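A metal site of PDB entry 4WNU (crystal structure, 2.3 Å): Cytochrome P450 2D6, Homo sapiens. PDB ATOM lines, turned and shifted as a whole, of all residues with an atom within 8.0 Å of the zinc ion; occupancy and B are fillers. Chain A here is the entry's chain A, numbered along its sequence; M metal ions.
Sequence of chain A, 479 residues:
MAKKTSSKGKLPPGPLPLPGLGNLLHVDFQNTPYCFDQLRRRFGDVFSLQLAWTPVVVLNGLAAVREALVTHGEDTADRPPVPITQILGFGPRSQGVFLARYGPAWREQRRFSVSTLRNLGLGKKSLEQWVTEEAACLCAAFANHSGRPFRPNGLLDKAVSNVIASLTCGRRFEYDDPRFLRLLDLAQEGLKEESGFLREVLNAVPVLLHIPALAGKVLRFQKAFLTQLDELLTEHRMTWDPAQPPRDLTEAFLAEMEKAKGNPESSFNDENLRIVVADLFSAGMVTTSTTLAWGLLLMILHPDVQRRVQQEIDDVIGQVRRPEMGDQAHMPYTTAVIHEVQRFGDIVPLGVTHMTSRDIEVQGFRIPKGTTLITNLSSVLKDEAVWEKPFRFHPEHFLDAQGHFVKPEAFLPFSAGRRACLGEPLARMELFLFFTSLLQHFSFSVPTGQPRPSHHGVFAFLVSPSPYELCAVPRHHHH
The side-chain carboxylate (OE1) of Glu 251 lies within hydrogen-bond range of the backbone NH (N) of Arg 247. A ring nitrogen (NE2) of His 236 lies close to the backbone carbonyl oxygen of Cys 169 (3.3 Å). O of His 236 is in hydrogen-bond range of OG1 of Thr 239, 3.2 Å away. The backbone NH (N) of Gly 170 lies close to the side-chain carboxylate (OD2) of Asp 248 (3.1 Å). OG1 of Thr 168 is in hydrogen-bond range of SG of Cys 169 (3.8 Å).
Residues that only touch the zinc ion: Cys 169 (3.4 Å). Four residues have an atom within 4 Å of the zinc ion: Cys 169, His 236, Asp 248 and Glu 251. The nearest printed residue that does not touch the zinc ion is Arg 247 (4.3 Å).
The zinc ion is bound by the side-chain carboxylate of Glu 251 (1.8 Å), a ring nitrogen (NE2) of His 236 (1.9 Å) and the side-chain carboxylate of Asp 248 (2.2 Å).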
ATOM      1  N   ALA A 165       4.188 -10.474 -13.825  1.00  0.00           N
ATOM      2  CA  ALA A 165       3.948 -10.895 -12.451  1.00  0.00           C
ATOM      3  C   ALA A 165       4.063  -9.692 -11.542  1.00  0.00           C
ATOM      4  O   ALA A 165       3.259  -9.504 -10.642  1.00  0.00           O
ATOM      5  CB  ALA A 165       4.950 -12.025 -12.029  1.00  0.00           C
ATOM      6  N   SER A 166       5.079  -8.862 -11.794  1.00  0.00           N
ATOM      7  CA  SER A 166       5.279  -7.662 -10.992  1.00  0.00           C
ATOM      8  C   SER A 166       4.136  -6.657 -11.143  1.00  0.00           C
ATOM      9  O   SER A 166       3.667  -6.102 -10.154  1.00  0.00           O
ATOM     10  CB  SER A 166       6.599  -6.988 -11.367  1.00  0.00           C
ATOM     11  OG  SER A 166       7.680  -7.810 -10.962  1.00  0.00           O
ATOM     12  N   LEU A 167       3.714  -6.425 -12.383  1.00  0.00           N
ATOM     13  CA  LEU A 167       2.603  -5.516 -12.677  1.00  0.00           C
ATOM     14  C   LEU A 167       1.286  -6.002 -12.075  1.00  0.00           C
ATOM     15  O   LEU A 167       0.479  -5.196 -11.601  1.00  0.00           O
ATOM     16  CB  LEU A 167       2.444  -5.354 -14.196  1.00  0.00           C
ATOM     17  CG  LEU A 167       1.071  -4.939 -14.738  1.00  0.00           C
ATOM     18  CD1 LEU A 167       0.730  -3.478 -14.379  1.00  0.00           C
ATOM     19  CD2 LEU A 167       0.987  -5.149 -16.265  1.00  0.00           C
ATOM     20  N   THR A 168       1.065  -7.320 -12.122  1.00  0.00           N
ATOM     21  CA  THR A 168      -0.252  -7.850 -11.814  1.00  0.00           C
ATOM     22  C   THR A 168      -0.369  -8.249 -10.355  1.00  0.00           C
ATOM     23  O   THR A 168      -1.401  -7.981  -9.739  1.00  0.00           O
ATOM     24  CB  THR A 168      -0.628  -9.061 -12.674  1.00  0.00           C
ATOM     25  OG1 THR A 168       0.346 -10.102 -12.513  1.00  0.00           O
ATOM     26  CG2 THR A 168      -0.765  -8.656 -14.141  1.00  0.00           C
ATOM     27  N   CYS A 169       0.680  -8.872  -9.810  1.00  0.00           N
ATOM     28  CA  CYS A 169       0.650  -9.365  -8.445  1.00  0.00           C
ATOM     29  C   CYS A 169       1.672  -8.693  -7.534  1.00  0.00           C
ATOM     30  O   CYS A 169       1.732  -9.017  -6.373  1.00  0.00           O
ATOM     31  CB  CYS A 169       0.889 -10.881  -8.397  1.00  0.00           C
ATOM     32  SG  CYS A 169      -0.235 -11.980  -9.317  1.00  0.00           S
ATOM     33  N   GLY A 170       2.493  -7.785  -8.055  1.00  0.00           N
ATOM     34  CA  GLY A 170       3.500  -7.156  -7.219  1.00  0.00           C
ATOM     35  C   GLY A 170       4.546  -8.122  -6.636  1.00  0.00           C
ATOM     36  O   GLY A 170       5.002  -7.952  -5.491  1.00  0.00           O
ATOM     37  N   ARG A 171       4.926  -9.124  -7.420  1.00  0.00           N
ATOM     38  CA  ARG A 171       6.022 -10.044  -7.028  1.00  0.00           C
ATOM     39  C   ARG A 171       6.684 -10.618  -8.262  1.00  0.00           C
ATOM     40  O   ARG A 171       6.076 -10.616  -9.339  1.00  0.00           O
ATOM     41  CB  ARG A 171       5.514 -11.202  -6.174  1.00  0.00           C
ATOM     42  CG  ARG A 171       4.614 -12.161  -6.946  1.00  0.00           C
ATOM     43  CD  ARG A 171       4.469 -13.513  -6.281  1.00  0.00           C
ATOM     44  NE  ARG A 171       5.751 -14.214  -6.196  1.00  0.00           N
ATOM     45  CZ  ARG A 171       5.943 -15.332  -5.522  1.00  0.00           C
ATOM     46  NH1 ARG A 171       4.943 -15.881  -4.835  1.00  0.00           N
ATOM     47  NH2 ARG A 171       7.145 -15.903  -5.485  1.00  0.00           N
ATOM     48  N   HIS A 236      -2.470 -13.893  -3.243  1.00  0.00           N
ATOM     49  CA  HIS A 236      -2.279 -12.456  -3.263  1.00  0.00           C
ATOM     50  C   HIS A 236      -3.402 -11.754  -2.515  1.00  0.00           C
ATOM     51  O   HIS A 236      -3.194 -10.745  -1.876  1.00  0.00           O
ATOM     52  CB  HIS A 236      -2.224 -11.961  -4.707  1.00  0.00           C
ATOM     53  CG  HIS A 236      -1.885 -10.511  -4.842  1.00  0.00           C
ATOM     54  ND1 HIS A 236      -2.570  -9.679  -5.687  1.00  0.00           N
ATOM     55  CD2 HIS A 236      -0.952  -9.750  -4.232  1.00  0.00           C
ATOM     56  CE1 HIS A 236      -2.055  -8.463  -5.613  1.00  0.00           C
ATOM     57  NE2 HIS A 236      -1.081  -8.471  -4.736  1.00  0.00           N
ATOM     58  N   ARG A 237      -4.602 -12.334  -2.570  1.00  0.00           N
ATOM     59  CA  ARG A 237      -5.739 -11.667  -1.978  1.00  0.00           C
ATOM     60  C   ARG A 237      -5.598 -11.714  -0.463  1.00  0.00           C
ATOM     61  O   ARG A 237      -6.084 -10.823   0.231  1.00  0.00           O
ATOM     62  CB  ARG A 237      -7.057 -12.287  -2.452  1.00  0.00           C
ATOM     63  CG  ARG A 237      -8.266 -11.757  -1.724  1.00  0.00           C
ATOM     64  CD  ARG A 237      -9.493 -11.594  -2.600  1.00  0.00           C
ATOM     65  NE  ARG A 237      -9.513 -12.503  -3.741  1.00  0.00           N
ATOM     66  CZ  ARG A 237     -10.476 -12.512  -4.654  1.00  0.00           C
ATOM     67  NH1 ARG A 237     -11.489 -11.661  -4.536  1.00  0.00           N
ATOM     68  NH2 ARG A 237     -10.435 -13.353  -5.693  1.00  0.00           N
ATOM     69  N   THR A 239      -2.608 -11.392   1.084  1.00  0.00           N
ATOM     70  CA  THR A 239      -1.564 -10.468   1.512  1.00  0.00           C
ATOM     71  C   THR A 239      -1.830  -8.989   1.178  1.00  0.00           C
ATOM     72  O   THR A 239      -1.106  -8.129   1.654  1.00  0.00           O
ATOM     73  CB  THR A 239      -0.203 -10.836   0.894  1.00  0.00           C
ATOM     74  OG1 THR A 239      -0.301 -10.782  -0.523  1.00  0.00           O
ATOM     75  CG2 THR A 239       0.222 -12.223   1.348  1.00  0.00           C
ATOM     76  N   TRP A 240      -2.822  -8.717   0.329  1.00  0.00           N
ATOM     77  CA  TRP A 240      -3.299  -7.349   0.059  1.00  0.00           C
ATOM     78  C   TRP A 240      -3.477  -6.518   1.331  1.00  0.00           C
ATOM     79  O   TRP A 240      -4.150  -6.964   2.270  1.00  0.00           O
ATOM     80  CB  TRP A 240      -4.634  -7.396  -0.679  1.00  0.00           C
ATOM     81  CG  TRP A 240      -5.242  -6.068  -1.045  1.00  0.00           C
ATOM     82  CD1 TRP A 240      -4.575  -4.898  -1.273  1.00  0.00           C
ATOM     83  CD2 TRP A 240      -6.629  -5.780  -1.246  1.00  0.00           C
ATOM     84  NE1 TRP A 240      -5.469  -3.899  -1.602  1.00  0.00           N
ATOM     85  CE2 TRP A 240      -6.739  -4.420  -1.591  1.00  0.00           C
ATOM     86  CE3 TRP A 240      -7.797  -6.541  -1.139  1.00  0.00           C
ATOM     87  CZ2 TRP A 240      -7.959  -3.798  -1.842  1.00  0.00           C
ATOM     88  CZ3 TRP A 240      -9.013  -5.936  -1.395  1.00  0.00           C
ATOM     89  CH2 TRP A 240      -9.082  -4.567  -1.746  1.00  0.00           C
ATOM     90  N   ASP A 241      -2.874  -5.328   1.373  1.00  0.00           N
ATOM     91  CA  ASP A 241      -3.158  -4.354   2.435  1.00  0.00           C
ATOM     92  C   ASP A 241      -4.047  -3.235   1.899  1.00  0.00           C
ATOM     93  O   ASP A 241      -3.553  -2.262   1.334  1.00  0.00           O
ATOM     94  CB  ASP A 241      -1.863  -3.777   3.000  1.00  0.00           C
ATOM     95  CG  ASP A 241      -2.084  -3.016   4.291  1.00  0.00           C
ATOM     96  OD1 ASP A 241      -1.104  -2.544   4.905  1.00  0.00           O
ATOM     97  OD2 ASP A 241      -3.250  -2.885   4.675  1.00  0.00           O
ATOM     98  N   PRO A 245      -2.264   2.500  -0.483  1.00  0.00           N
ATOM     99  CA  PRO A 245      -2.485   2.613  -1.928  1.00  0.00           C
ATOM    100  C   PRO A 245      -2.128   1.304  -2.623  1.00  0.00           C
ATOM    101  O   PRO A 245      -1.250   0.603  -2.139  1.00  0.00           O
ATOM    102  CB  PRO A 245      -1.524   3.743  -2.336  1.00  0.00           C
ATOM    103  CG  PRO A 245      -1.485   4.614  -1.097  1.00  0.00           C
ATOM    104  CD  PRO A 245      -1.455   3.619   0.036  1.00  0.00           C
ATOM    105  N   PRO A 246      -2.848   0.962  -3.701  1.00  0.00           N
ATOM    106  CA  PRO A 246      -2.568  -0.301  -4.399  1.00  0.00           C
ATOM    107  C   PRO A 246      -1.129  -0.402  -4.888  1.00  0.00           C
ATOM    108  O   PRO A 246      -0.624   0.555  -5.490  1.00  0.00           O
ATOM    109  CB  PRO A 246      -3.557  -0.263  -5.562  1.00  0.00           C
ATOM    110  CG  PRO A 246      -4.711   0.577  -5.055  1.00  0.00           C
ATOM    111  CD  PRO A 246      -4.078   1.615  -4.180  1.00  0.00           C
ATOM    112  N   ARG A 247      -0.486  -1.541  -4.643  1.00  0.00           N
ATOM    113  CA  ARG A 247       0.903  -1.763  -5.058  1.00  0.00           C
ATOM    114  C   ARG A 247       1.026  -2.281  -6.490  1.00  0.00           C
ATOM    115  O   ARG A 247       2.094  -2.302  -7.072  1.00  0.00           O
ATOM    116  CB  ARG A 247       1.580  -2.787  -4.135  1.00  0.00           C
ATOM    117  CG  ARG A 247       2.025  -2.303  -2.780  1.00  0.00           C
ATOM    118  CD  ARG A 247       3.310  -3.027  -2.382  1.00  0.00           C
ATOM    119  NE  ARG A 247       3.315  -4.387  -2.924  1.00  0.00           N
ATOM    120  CZ  ARG A 247       4.225  -4.891  -3.765  1.00  0.00           C
ATOM    121  NH1 ARG A 247       5.256  -4.156  -4.178  1.00  0.00           N
ATOM    122  NH2 ARG A 247       4.089  -6.131  -4.188  1.00  0.00           N
ATOM    123  N   ASP A 248      -0.090  -2.757  -7.041  1.00  0.00           N
ATOM    124  CA  ASP A 248      -0.101  -3.417  -8.320  1.00  0.00           C
ATOM    125  C   ASP A 248      -1.508  -3.434  -8.827  1.00  0.00           C
ATOM    126  O   ASP A 248      -2.413  -3.007  -8.135  1.00  0.00           O
ATOM    127  CB  ASP A 248       0.442  -4.843  -8.220  1.00  0.00           C
ATOM    128  CG  ASP A 248      -0.153  -5.601  -7.065  1.00  0.00           C
ATOM    129  OD1 ASP A 248      -1.389  -5.717  -6.947  1.00  0.00           O
ATOM    130  OD2 ASP A 248       0.628  -6.088  -6.238  1.00  0.00           O
ATOM    131  N   LEU A 249      -1.686  -3.977 -10.020  1.00  0.00           N
ATOM    132  CA  LEU A 249      -2.930  -3.877 -10.775  1.00  0.00           C
ATOM    133  C   LEU A 249      -4.044  -4.732 -10.190  1.00  0.00           C
ATOM    134  O   LEU A 249      -5.202  -4.301 -10.183  1.00  0.00           O
ATOM    135  CB  LEU A 249      -2.664  -4.247 -12.256  1.00  0.00           C
ATOM    136  CG  LEU A 249      -3.856  -4.226 -13.228  1.00  0.00           C
ATOM    137  CD1 LEU A 249      -3.488  -3.734 -14.638  1.00  0.00           C
ATOM    138  CD2 LEU A 249      -4.528  -5.595 -13.348  1.00  0.00           C
ATOM    139  N   THR A 250      -3.718  -5.932  -9.705  1.00  0.00           N
ATOM    140  CA  THR A 250      -4.720  -6.769  -9.026  1.00  0.00           C
ATOM    141  C   THR A 250      -5.296  -6.032  -7.804  1.00  0.00           C
ATOM    142  O   THR A 250      -6.502  -6.074  -7.532  1.00  0.00           O
ATOM    143  CB  THR A 250      -4.104  -8.158  -8.617  1.00  0.00           C
ATOM    144  OG1 THR A 250      -3.845  -8.934  -9.809  1.00  0.00           O
ATOM    145  CG2 THR A 250      -5.005  -8.946  -7.700  1.00  0.00           C
ATOM    146  N   GLU A 251      -4.445  -5.322  -7.072  1.00  0.00           N
ATOM    147  CA  GLU A 251      -4.906  -4.605  -5.894  1.00  0.00           C
ATOM    148  C   GLU A 251      -5.790  -3.431  -6.283  1.00  0.00           C
ATOM    149  O   GLU A 251      -6.784  -3.136  -5.599  1.00  0.00           O
ATOM    150  CB  GLU A 251      -3.725  -4.137  -5.038  1.00  0.00           C
ATOM    151  CG  GLU A 251      -3.019  -5.328  -4.298  1.00  0.00           C
ATOM    152  CD  GLU A 251      -1.796  -4.882  -3.531  1.00  0.00           C
ATOM    153  OE1 GLU A 251      -1.706  -3.670  -3.224  1.00  0.00           O
ATOM    154  OE2 GLU A 251      -0.944  -5.760  -3.207  1.00  0.00           O
ATOM    155  N   ALA A 252      -5.430  -2.765  -7.378  1.00  0.00           N
ATOM    156  CA  ALA A 252      -6.263  -1.668  -7.872  1.00  0.00           C
ATOM    157  C   ALA A 252      -7.646  -2.209  -8.260  1.00  0.00           C
ATOM    158  O   ALA A 252      -8.664  -1.602  -7.960  1.00  0.00           O
ATOM    159  CB  ALA A 252      -5.585  -0.957  -9.055  1.00  0.00           C
ATOM    160  N   LEU A 254      -9.104  -5.037  -7.118  1.00  0.00           N
ATOM    161  CA  LEU A 254      -9.785  -5.531  -5.922  1.00  0.00           C
ATOM    162  C   LEU A 254     -10.480  -4.353  -5.238  1.00  0.00           C
ATOM    163  O   LEU A 254     -11.644  -4.449  -4.877  1.00  0.00           O
ATOM    164  CB  LEU A 254      -8.818  -6.250  -4.961  1.00  0.00           C
ATOM    165  CG  LEU A 254      -8.421  -7.675  -5.360  1.00  0.00           C
ATOM    166  CD1 LEU A 254      -7.202  -8.137  -4.583  1.00  0.00           C
ATOM    167  CD2 LEU A 254      -9.563  -8.674  -5.216  1.00  0.00           C
HETATM  168 ZN    ZN M   1      -0.097  -6.900  -4.372  1.00  0.00          ZN
